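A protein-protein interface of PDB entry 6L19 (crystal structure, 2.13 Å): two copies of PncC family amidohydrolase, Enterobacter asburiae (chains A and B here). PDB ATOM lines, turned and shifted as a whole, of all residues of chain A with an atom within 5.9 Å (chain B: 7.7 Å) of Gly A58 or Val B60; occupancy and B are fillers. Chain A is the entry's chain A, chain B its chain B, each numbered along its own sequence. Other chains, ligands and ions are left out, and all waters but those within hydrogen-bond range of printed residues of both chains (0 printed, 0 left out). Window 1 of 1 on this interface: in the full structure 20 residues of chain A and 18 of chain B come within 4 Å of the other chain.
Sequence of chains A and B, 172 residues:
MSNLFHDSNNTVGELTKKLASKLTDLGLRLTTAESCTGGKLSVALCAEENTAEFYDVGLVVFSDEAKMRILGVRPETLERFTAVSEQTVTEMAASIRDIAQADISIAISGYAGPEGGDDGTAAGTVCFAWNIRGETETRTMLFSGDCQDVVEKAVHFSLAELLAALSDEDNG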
ATOM      1  N   THR A  31     -11.456 -35.823   3.243  1.00  0.00           N
ATOM      2  CA  THR A  31     -11.854 -35.229   1.978  1.00  0.00           C
ATOM      3  C   THR A  31     -13.292 -35.646   1.710  1.00  0.00           C
ATOM      4  O   THR A  31     -13.770 -36.644   2.259  1.00  0.00           O
ATOM      5  CB  THR A  31     -10.933 -35.676   0.827  1.00  0.00           C
ATOM      6  OG1 THR A  31     -11.303 -34.986  -0.374  1.00  0.00           O
ATOM      7  CG2 THR A  31     -11.075 -37.190   0.598  1.00  0.00           C
ATOM      8  N   THR A  32     -13.986 -34.878   0.864  1.00  0.00           N
ATOM      9  CA  THR A  32     -15.403 -35.105   0.609  1.00  0.00           C
ATOM     10  C   THR A  32     -15.742 -34.955  -0.869  1.00  0.00           C
ATOM     11  O   THR A  32     -15.167 -34.128  -1.583  1.00  0.00           O
ATOM     12  CB  THR A  32     -16.304 -34.117   1.388  1.00  0.00           C
ATOM     13  OG1 THR A  32     -15.960 -32.774   1.015  1.00  0.00           O
ATOM     14  CG2 THR A  32     -16.139 -34.290   2.869  1.00  0.00           C
ATOM     15  N   ALA A  33     -16.746 -35.715  -1.299  1.00  0.00           N
ATOM     16  CA  ALA A  33     -17.337 -35.560  -2.626  1.00  0.00           C
ATOM     17  C   ALA A  33     -18.854 -35.563  -2.486  1.00  0.00           C
ATOM     18  O   ALA A  33     -19.436 -36.533  -1.985  1.00  0.00           O
ATOM     19  CB  ALA A  33     -16.871 -36.672  -3.570  1.00  0.00           C
ATOM     20  N   SER A  42     -18.861 -29.398   2.647  1.00  0.00           N
ATOM     21  CA  SER A  42     -17.589 -28.679   2.611  1.00  0.00           C
ATOM     22  C   SER A  42     -17.626 -27.423   3.484  1.00  0.00           C
ATOM     23  O   SER A  42     -16.694 -27.161   4.257  1.00  0.00           O
ATOM     24  CB  SER A  42     -17.261 -28.312   1.167  1.00  0.00           C
ATOM     25  OG  SER A  42     -16.004 -27.688   1.103  1.00  0.00           O
ATOM     26  N   CYS A  46     -15.217 -26.497   6.565  1.00  0.00           N
ATOM     27  CA  CYS A  46     -14.355 -25.327   6.492  1.00  0.00           C
ATOM     28  C   CYS A  46     -14.684 -24.302   7.576  1.00  0.00           C
ATOM     29  O   CYS A  46     -13.856 -23.434   7.867  1.00  0.00           O
ATOM     30  CB  CYS A  46     -14.484 -24.701   5.104  1.00  0.00           C
ATOM     31  SG  CYS A  46     -13.624 -25.641   3.814  1.00  0.00           S
ATOM     32  N   TYR A  55      -8.603 -30.918   6.861  1.00  0.00           N
ATOM     33  CA  TYR A  55      -9.486 -30.892   5.700  1.00  0.00           C
ATOM     34  C   TYR A  55      -8.845 -30.074   4.595  1.00  0.00           C
ATOM     35  O   TYR A  55      -8.444 -28.928   4.820  1.00  0.00           O
ATOM     36  CB  TYR A  55     -10.862 -30.303   6.059  1.00  0.00           C
ATOM     37  CG  TYR A  55     -11.862 -30.362   4.926  1.00  0.00           C
ATOM     38  CD1 TYR A  55     -12.280 -31.584   4.399  1.00  0.00           C
ATOM     39  CD2 TYR A  55     -12.382 -29.205   4.374  1.00  0.00           C
ATOM     40  CE1 TYR A  55     -13.185 -31.649   3.366  1.00  0.00           C
ATOM     41  CE2 TYR A  55     -13.304 -29.264   3.340  1.00  0.00           C
ATOM     42  CZ  TYR A  55     -13.697 -30.495   2.841  1.00  0.00           C
ATOM     43  OH  TYR A  55     -14.605 -30.574   1.816  1.00  0.00           O
ATOM     44  N   ASP A  56      -8.771 -30.647   3.400  1.00  0.00           N
ATOM     45  CA  ASP A  56      -8.100 -29.976   2.299  1.00  0.00           C
ATOM     46  C   ASP A  56      -9.026 -29.867   1.091  1.00  0.00           C
ATOM     47  O   ASP A  56      -9.388 -28.754   0.685  1.00  0.00           O
ATOM     48  CB  ASP A  56      -6.811 -30.724   1.953  1.00  0.00           C
ATOM     49  CG  ASP A  56      -5.921 -29.971   0.961  1.00  0.00           C
ATOM     50  OD1 ASP A  56      -6.262 -28.845   0.525  1.00  0.00           O
ATOM     51  OD2 ASP A  56      -4.856 -30.528   0.625  1.00  0.00           O
ATOM     52  N   VAL A  57      -9.449 -31.003   0.538  1.00  0.00           N
ATOM     53  CA  VAL A  57     -10.109 -31.053  -0.761  1.00  0.00           C
ATOM     54  C   VAL A  57     -11.585 -31.413  -0.595  1.00  0.00           C
ATOM     55  O   VAL A  57     -11.929 -32.402   0.069  1.00  0.00           O
ATOM     56  CB  VAL A  57      -9.407 -32.060  -1.695  1.00  0.00           C
ATOM     57  CG1 VAL A  57     -10.217 -32.248  -2.958  1.00  0.00           C
ATOM     58  CG2 VAL A  57      -7.997 -31.580  -2.014  1.00  0.00           C
ATOM     59  N   GLY A  58     -12.451 -30.623  -1.221  1.00  0.00           N
ATOM     60  CA  GLY A  58     -13.863 -30.952  -1.320  1.00  0.00           C
ATOM     61  C   GLY A  58     -14.304 -30.838  -2.762  1.00  0.00           C
ATOM     62  O   GLY A  58     -13.961 -29.872  -3.449  1.00  0.00           O
ATOM     63  N   LEU A  59     -15.035 -31.822  -3.250  1.00  0.00           N
ATOM     64  CA  LEU A  59     -15.549 -31.784  -4.608  1.00  0.00           C
ATOM     65  C   LEU A  59     -17.067 -31.767  -4.589  1.00  0.00           C
ATOM     66  O   LEU A  59     -17.696 -32.447  -3.773  1.00  0.00           O
ATOM     67  CB  LEU A  59     -15.052 -32.994  -5.421  1.00  0.00           C
ATOM     68  CG  LEU A  59     -15.426 -32.940  -6.895  1.00  0.00           C
ATOM     69  CD1 LEU A  59     -14.572 -31.905  -7.594  1.00  0.00           C
ATOM     70  CD2 LEU A  59     -15.251 -34.350  -7.516  1.00  0.00           C
ATOM     71  N   VAL A  60     -17.647 -30.979  -5.489  1.00  0.00           N
ATOM     72  CA  VAL A  60     -19.086 -30.948  -5.734  1.00  0.00           C
ATOM     73  C   VAL A  60     -19.304 -31.291  -7.205  1.00  0.00           C
ATOM     74  O   VAL A  60     -18.664 -30.692  -8.078  1.00  0.00           O
ATOM     75  CB  VAL A  60     -19.680 -29.561  -5.410  1.00  0.00           C
ATOM     76  CG1 VAL A  60     -21.140 -29.496  -5.820  1.00  0.00           C
ATOM     77  CG2 VAL A  60     -19.523 -29.232  -3.925  1.00  0.00           C
ATOM     78  N   ILE A  96     -12.078 -39.940  -4.651  1.00  0.00           N
ATOM     79  CA  ILE A  96     -11.749 -38.656  -4.030  1.00  0.00           C
ATOM     80  C   ILE A  96     -10.675 -38.838  -2.963  1.00  0.00           C
ATOM     81  O   ILE A  96      -9.813 -37.969  -2.782  1.00  0.00           O
ATOM     82  CB  ILE A  96     -13.013 -37.968  -3.457  1.00  0.00           C
ATOM     83  CG1 ILE A  96     -12.707 -36.498  -3.124  1.00  0.00           C
ATOM     84  CG2 ILE A  96     -13.536 -38.706  -2.199  1.00  0.00           C
ATOM     85  CD1 ILE A  96     -12.312 -35.638  -4.342  1.00  0.00           C
ATOM     86  N   THR B  32     -16.211 -23.756 -10.780  1.00  0.00           N
ATOM     87  CA  THR B  32     -15.574 -22.925  -9.759  1.00  0.00           C
ATOM     88  C   THR B  32     -14.486 -23.685  -9.016  1.00  0.00           C
ATOM     89  O   THR B  32     -14.612 -24.888  -8.765  1.00  0.00           O
ATOM     90  CB  THR B  32     -16.594 -22.410  -8.708  1.00  0.00           C
ATOM     91  OG1 THR B  32     -17.226 -23.527  -8.057  1.00  0.00           O
ATOM     92  CG2 THR B  32     -17.660 -21.521  -9.355  1.00  0.00           C
ATOM     93  N   ALA B  33     -13.435 -22.956  -8.622  1.00  0.00           N
ATOM     94  CA  ALA B  33     -12.373 -23.459  -7.751  1.00  0.00           C
ATOM     95  C   ALA B  33     -12.151 -22.465  -6.616  1.00  0.00           C
ATOM     96  O   ALA B  33     -11.792 -21.311  -6.864  1.00  0.00           O
ATOM     97  CB  ALA B  33     -11.073 -23.676  -8.536  1.00  0.00           C
ATOM     98  N   GLU B  34     -12.349 -22.909  -5.373  1.00  0.00           N
ATOM     99  CA  GLU B  34     -12.392 -22.028  -4.204  1.00  0.00           C
ATOM    100  C   GLU B  34     -11.265 -22.383  -3.245  1.00  0.00           C
ATOM    101  O   GLU B  34     -11.215 -23.503  -2.718  1.00  0.00           O
ATOM    102  CB  GLU B  34     -13.729 -22.155  -3.460  1.00  0.00           C
ATOM    103  CG  GLU B  34     -14.949 -21.730  -4.196  1.00  0.00           C
ATOM    104  CD  GLU B  34     -16.212 -22.012  -3.378  1.00  0.00           C
ATOM    105  OE1 GLU B  34     -16.368 -21.411  -2.279  1.00  0.00           O
ATOM    106  OE2 GLU B  34     -17.033 -22.843  -3.828  1.00  0.00           O
ATOM    107  N   SER B  35     -10.388 -21.430  -2.988  1.00  0.00           N
ATOM    108  CA  SER B  35      -9.338 -21.589  -1.994  1.00  0.00           C
ATOM    109  C   SER B  35      -9.370 -20.397  -1.033  1.00  0.00           C
ATOM    110  O   SER B  35      -8.421 -19.602  -0.987  1.00  0.00           O
ATOM    111  CB  SER B  35      -7.975 -21.726  -2.645  1.00  0.00           C
ATOM    112  OG  SER B  35      -7.043 -21.920  -1.613  1.00  0.00           O
ATOM    113  N   CYS B  36     -10.437 -20.321  -0.230  1.00  0.00           N
ATOM    114  CA  CYS B  36     -10.675 -19.170   0.627  1.00  0.00           C
ATOM    115  C   CYS B  36     -12.094 -19.228   1.190  1.00  0.00           C
ATOM    116  O   CYS B  36     -12.309 -19.160   2.401  1.00  0.00           O
ATOM    117  CB  CYS B  36     -10.448 -17.895  -0.197  1.00  0.00           C
ATOM    118  SG  CYS B  36     -10.927 -16.428   0.486  1.00  0.00           S
ATOM    119  N   THR B  37     -13.059 -19.387   0.304  1.00  0.00           N
ATOM    120  CA  THR B  37     -14.474 -19.284   0.619  1.00  0.00           C
ATOM    121  C   THR B  37     -15.104 -20.599   1.069  1.00  0.00           C
ATOM    122  O   THR B  37     -16.298 -20.612   1.371  1.00  0.00           O
ATOM    123  CB  THR B  37     -15.203 -18.750  -0.604  1.00  0.00           C
ATOM    124  OG1 THR B  37     -14.788 -19.509  -1.751  1.00  0.00           O
ATOM    125  CG2 THR B  37     -14.820 -17.287  -0.820  1.00  0.00           C
ATOM    126  N   GLY B  38     -14.354 -21.707   1.072  1.00  0.00           N
ATOM    127  CA  GLY B  38     -14.788 -22.919   1.743  1.00  0.00           C
ATOM    128  C   GLY B  38     -15.968 -23.646   1.128  1.00  0.00           C
ATOM    129  O   GLY B  38     -16.541 -24.519   1.775  1.00  0.00           O
ATOM    130  N   GLY B  39     -16.342 -23.335  -0.110  1.00  0.00           N
ATOM    131  CA  GLY B  39     -17.511 -23.942  -0.722  1.00  0.00           C
ATOM    132  C   GLY B  39     -18.738 -23.058  -0.734  1.00  0.00           C
ATOM    133  O   GLY B  39     -19.765 -23.451  -1.304  1.00  0.00           O
ATOM    134  N   LYS B  40     -18.664 -21.879  -0.113  1.00  0.00           N
ATOM    135  CA  LYS B  40     -19.811 -20.978  -0.095  1.00  0.00           C
ATOM    136  C   LYS B  40     -20.199 -20.529  -1.501  1.00  0.00           C
ATOM    137  O   LYS B  40     -21.380 -20.295  -1.772  1.00  0.00           O
ATOM    138  CB  LYS B  40     -19.499 -19.767   0.790  1.00  0.00           C
ATOM    139  CG  LYS B  40     -19.445 -20.103   2.292  1.00  0.00           C
ATOM    140  CD  LYS B  40     -20.770 -19.793   2.927  1.00  0.00           C
ATOM    141  CE  LYS B  40     -20.679 -19.712   4.429  1.00  0.00           C
ATOM    142  NZ  LYS B  40     -22.017 -20.083   4.981  1.00  0.00           N
ATOM    143  N   LEU B  41     -19.229 -20.386  -2.402  1.00  0.00           N
ATOM    144  CA  LEU B  41     -19.584 -20.032  -3.771  1.00  0.00           C
ATOM    145  C   LEU B  41     -20.354 -21.171  -4.436  1.00  0.00           C
ATOM    146  O   LEU B  41     -21.403 -20.955  -5.053  1.00  0.00           O
ATOM    147  CB  LEU B  41     -18.330 -19.667  -4.566  1.00  0.00           C
ATOM    148  CG  LEU B  41     -18.555 -19.421  -6.066  1.00  0.00           C
ATOM    149  CD1 LEU B  41     -19.552 -18.272  -6.285  1.00  0.00           C
ATOM    150  CD2 LEU B  41     -17.218 -19.139  -6.743  1.00  0.00           C
ATOM    151  N   SER B  42     -19.859 -22.400  -4.300  1.00  0.00           N
ATOM    152  CA  SER B  42     -20.616 -23.563  -4.764  1.00  0.00           C
ATOM    153  C   SER B  42     -22.042 -23.583  -4.202  1.00  0.00           C
ATOM    154  O   SER B  42     -23.017 -23.796  -4.935  1.00  0.00           O
ATOM    155  CB  SER B  42     -19.877 -24.834  -4.359  1.00  0.00           C
ATOM    156  OG  SER B  42     -20.343 -25.915  -5.126  1.00  0.00           O
ATOM    157  N   TYR B  55     -24.371 -25.389 -14.071  1.00  0.00           N
ATOM    158  CA  TYR B  55     -23.291 -25.536 -13.101  1.00  0.00           C
ATOM    159  C   TYR B  55     -23.191 -26.999 -12.726  1.00  0.00           C
ATOM    160  O   TYR B  55     -24.198 -27.608 -12.353  1.00  0.00           O
ATOM    161  CB  TYR B  55     -23.553 -24.682 -11.849  1.00  0.00           C
ATOM    162  CG  TYR B  55     -22.465 -24.724 -10.785  1.00  0.00           C
ATOM    163  CD1 TYR B  55     -21.173 -24.282 -11.057  1.00  0.00           C
ATOM    164  CD2 TYR B  55     -22.741 -25.182  -9.504  1.00  0.00           C
ATOM    165  CE1 TYR B  55     -20.179 -24.292 -10.079  1.00  0.00           C
ATOM    166  CE2 TYR B  55     -21.753 -25.205  -8.513  1.00  0.00           C
ATOM    167  CZ  TYR B  55     -20.480 -24.757  -8.807  1.00  0.00           C
ATOM    168  OH  TYR B  55     -19.515 -24.783  -7.844  1.00  0.00           O
ATOM    169  N   GLY B  58     -17.809 -28.038  -8.803  1.00  0.00           N
ATOM    170  CA  GLY B  58     -17.142 -27.076  -7.937  1.00  0.00           C
ATOM    171  C   GLY B  58     -16.070 -27.764  -7.126  1.00  0.00           C
ATOM    172  O   GLY B  58     -16.280 -28.859  -6.590  1.00  0.00           O
ATOM    173  N   LEU B  59     -14.906 -27.116  -7.044  1.00  0.00           N
ATOM    174  CA  LEU B  59     -13.773 -27.616  -6.285  1.00  0.00           C
ATOM    175  C   LEU B  59     -13.454 -26.677  -5.121  1.00  0.00           C
ATOM    176  O   LEU B  59     -13.520 -25.447  -5.251  1.00  0.00           O
ATOM    177  CB  LEU B  59     -12.541 -27.782  -7.196  1.00  0.00           C
ATOM    178  CG  LEU B  59     -11.283 -28.319  -6.491  1.00  0.00           C
ATOM    179  CD1 LEU B  59     -11.471 -29.764  -6.085  1.00  0.00           C
ATOM    180  CD2 LEU B  59     -10.040 -28.158  -7.352  1.00  0.00           C
ATOM    181  N   VAL B  60     -13.129 -27.271  -3.976  1.00  0.00           N
ATOM    182  CA  VAL B  60     -12.627 -26.566  -2.805  1.00  0.00           C
ATOM    183  C   VAL B  60     -11.264 -27.165  -2.480  1.00  0.00           C
ATOM    184  O   VAL B  60     -11.143 -28.390  -2.365  1.00  0.00           O
ATOM    185  CB  VAL B  60     -13.597 -26.705  -1.612  1.00  0.00           C
ATOM    186  CG1 VAL B  60     -13.012 -26.065  -0.342  1.00  0.00           C
ATOM    187  CG2 VAL B  60     -14.946 -26.099  -1.958  1.00  0.00           C
ATOM    188  N   VAL B  61     -10.237 -26.315  -2.360  1.00  0.00           N
ATOM    189  CA  VAL B  61      -8.888 -26.773  -2.011  1.00  0.00           C
ATOM    190  C   VAL B  61      -8.237 -25.768  -1.070  1.00  0.00           C
ATOM    191  O   VAL B  61      -8.363 -24.557  -1.253  1.00  0.00           O
ATOM    192  CB  VAL B  61      -7.981 -26.981  -3.248  1.00  0.00           C
ATOM    193  CG1 VAL B  61      -8.552 -28.021  -4.141  1.00  0.00           C
ATOM    194  CG2 VAL B  61      -7.789 -25.677  -4.026  1.00  0.00           C
ATOM    195  N   PHE B  62      -7.524 -26.272  -0.073  1.00  0.00           N
ATOM    196  CA  PHE B  62      -6.785 -25.413   0.841  1.00  0.00           C
ATOM    197  C   PHE B  62      -5.289 -25.351   0.530  1.00  0.00           C
ATOM    198  O   PHE B  62      -4.725 -24.258   0.478  1.00  0.00           O
ATOM    199  CB  PHE B  62      -6.993 -25.875   2.285  1.00  0.00           C
ATOM    200  CG  PHE B  62      -6.146 -25.125   3.278  1.00  0.00           C
ATOM    201  CD1 PHE B  62      -6.544 -23.880   3.745  1.00  0.00           C
ATOM    202  CD2 PHE B  62      -4.941 -25.656   3.729  1.00  0.00           C
ATOM    203  CE1 PHE B  62      -5.750 -23.177   4.651  1.00  0.00           C
ATOM    204  CE2 PHE B  62      -4.149 -24.965   4.630  1.00  0.00           C
ATOM    205  CZ  PHE B  62      -4.550 -23.723   5.087  1.00  0.00           C
ATOM    206  N   SER B  63      -4.642 -26.490   0.292  1.00  0.00           N
ATOM    207  CA  SER B  63      -3.181 -26.562   0.345  1.00  0.00           C
ATOM    208  C   SER B  63      -2.526 -26.154  -0.978  1.00  0.00           C
ATOM    209  O   SER B  63      -3.133 -26.203  -2.052  1.00  0.00           O
ATOM    210  CB  SER B  63      -2.732 -27.976   0.729  1.00  0.00           C
ATOM    211  OG  SER B  63      -2.969 -28.904  -0.324  1.00  0.00           O
ATOM    212  N   ALA B  66      -2.280 -29.460  -2.980  1.00  0.00           N
ATOM    213  CA  ALA B  66      -3.480 -29.772  -3.756  1.00  0.00           C
ATOM    214  C   ALA B  66      -3.585 -28.899  -5.000  1.00  0.00           C
ATOM    215  O   ALA B  66      -3.985 -29.378  -6.065  1.00  0.00           O
ATOM    216  CB  ALA B  66      -4.734 -29.621  -2.888  1.00  0.00           C
ATOM    217  N   ILE B  70      -3.770 -31.124  -8.177  1.00  0.00           N
ATOM    218  CA  ILE B  70      -5.082 -31.203  -8.819  1.00  0.00           C
ATOM    219  C   ILE B  70      -5.247 -30.151  -9.908  1.00  0.00           C
ATOM    220  O   ILE B  70      -5.863 -30.410 -10.946  1.00  0.00           O
ATOM    221  CB  ILE B  70      -6.212 -31.092  -7.777  1.00  0.00           C
ATOM    222  CG1 ILE B  70      -6.115 -32.193  -6.732  1.00  0.00           C
ATOM    223  CG2 ILE B  70      -7.589 -31.120  -8.466  1.00  0.00           C
ATOM    224  CD1 ILE B  70      -7.191 -32.050  -5.655  1.00  0.00           C
ATOM    225  N   LEU B  71      -4.761 -28.933  -9.700  1.00  0.00           N
ATOM    226  CA  LEU B  71      -5.046 -27.863 -10.650  1.00  0.00           C
ATOM    227  C   LEU B  71      -3.829 -27.490 -11.485  1.00  0.00           C
ATOM    228  O   LEU B  71      -3.860 -26.471 -12.184  1.00  0.00           O
ATOM    229  CB  LEU B  71      -5.600 -26.632  -9.924  1.00  0.00           C
ATOM    230  CG  LEU B  71      -6.993 -26.775  -9.315  1.00  0.00           C
ATOM    231  CD1 LEU B  71      -7.401 -25.511  -8.549  1.00  0.00           C
ATOM    232  CD2 LEU B  71      -8.032 -27.116 -10.383  1.00  0.00           C
ATOM    233  N   MET B  92      -5.284 -21.633 -11.644  1.00  0.00           N
ATOM    234  CA  MET B  92      -6.431 -22.363 -11.107  1.00  0.00           C
ATOM    235  C   MET B  92      -7.623 -22.263 -12.043  1.00  0.00           C
ATOM    236  O   MET B  92      -8.260 -23.268 -12.365  1.00  0.00           O
ATOM    237  CB  MET B  92      -6.835 -21.862  -9.712  1.00  0.00           C
ATOM    238  CG  MET B  92      -5.865 -22.170  -8.571  1.00  0.00           C
ATOM    239  SD  MET B  92      -6.206 -21.271  -7.020  1.00  0.00           S
ATOM    240  CE  MET B  92      -7.823 -21.895  -6.682  1.00  0.00           C
ATOM    241  N   ILE B  96      -9.344 -25.627 -13.877  1.00  0.00           N
ATOM    242  CA  ILE B  96     -10.660 -26.143 -13.517  1.00  0.00           C
ATOM    243  C   ILE B  96     -11.610 -26.031 -14.695  1.00  0.00           C
ATOM    244  O   ILE B  96     -12.498 -26.866 -14.853  1.00  0.00           O
ATOM    245  CB  ILE B  96     -11.221 -25.444 -12.255  1.00  0.00           C
ATOM    246  CG1 ILE B  96     -12.494 -26.161 -11.772  1.00  0.00           C
ATOM    247  CG2 ILE B  96     -11.536 -23.962 -12.525  1.00  0.00           C
ATOM    248  CD1 ILE B  96     -12.244 -27.587 -11.263  1.00  0.00           C
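The side-chain sulfur (SG) of Cys A46 sits close to the backbone carbonyl oxygen (O) of Gly B38.
The backbone NH (N) of Val A60 lies within hydrogen-bond range of the backbone carbonyl oxygen (O) of Gly B58, at 2.8 Å.
The side-chain carboxylate of Asp A56 sits at hydrogen-bond distance from the side-chain hydroxyl of Ser B63 (2.7 Å).
OD1 of Asp A56 is in hydrogen-bond range of N of Phe B62.
O of Gly A58 is in hydrogen-bond range of N of Val B60, 2.8 Å away.
The backbone carbonyl oxygen (O) of Gly B38 lies within hydrogen-bond range of the side-chain hydroxyl (OG) of Ser A42 (3.3 Å).
The side-chain carboxylate of Glu B34 lies within hydrogen-bond range of the backbone NH of Ser B42, at 2.9 Å.
The backbone carbonyl oxygen (O) of Val A57 sits at hydrogen-bond distance from the side-chain hydroxyl (OG1) of Thr A31, at 2.7 Å.
The backbone NH of Val B61 sits at hydrogen-bond distance from the backbone carbonyl oxygen of Glu B34.
The backbone carbonyl oxygen (O) of Ser A42 sits close to the side-chain sulfur (SG) of Cys A46 (3.5 Å).
The backbone NH (N) of Glu B34 lies within hydrogen-bond range of the backbone carbonyl oxygen (O) of Leu B59 (2.8 Å).
The side-chain hydroxyl (OG) of Ser B35 is in hydrogen-bond range of the backbone carbonyl oxygen (O) of Val B61.
OG of Ser A42 touches CG2 of Val B60, 3.6 Å away.
O of Asp A56 touches O of Val B60, 3.5 Å away.
Val B61 touches Asp A56 (CA to O, 3.4 Å).
Ala B66 touches Asp A56 (CB to OD2, 3.6 Å).
CA of Val A57 touches O of Val B60, at 3.3 Å.
Val A57 touches Ala B66.
Ile B70 touches Val A57 (CD1 to CG2, 3.8 Å).
CD1 of Leu B59 touches O of Gly A58 (3.6 Å).
CA of Leu A59 touches O of Gly B58, at 3.6 Å.
Val A60 touches Ser B42.
Gly A58 touches two residues of chain B.
Of the printed residues of chain A, Val B61 touches Asp A56 (3.4 Å).
Of the printed residues of chain A, Phe B62 touches Asp A56.
The nearest residue of chain A that does not touch Val B60 is Cys A46 (4.2 Å).
Printed residues of chain B that touch a printed residue of chain A: Gly B38, Ser B42, Gly B58, Leu B59, Val B60, Val B61, Phe B62, Ser B63, Ala B66 and Ile B70.
Hydrophobic or aromatic side chains of chain A within 4 Å of the printed part of chain B: Val A57, Leu A59 and Val A60.
Along chain A the printed residues that touch a printed residue of chain B span positions 42 to 60.
Among the printed residues, 16 pairs touch across the chains.
Among the printed residues, no Asp or Glu carboxylate lies within 4 Å of a Lys or Arg side-chain nitrogen of the other chain.
Ser A42 touches Val B60, and with the chains exchanged Val A60 touches Ser B42.
Gly A58 touches Leu B59, and with the chains exchanged Leu A59 touches Gly B58.
Gly A58 touches Val B60, and with the chains exchanged Val A60 touches Gly B58.
Positions printed for both chains: 32, 33, 42, 55, 58, 59, 60 and 96.
Of the 16 pairs that touch across the chains among the printed residues, 6 have their exchanged pair printed and touching as well.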
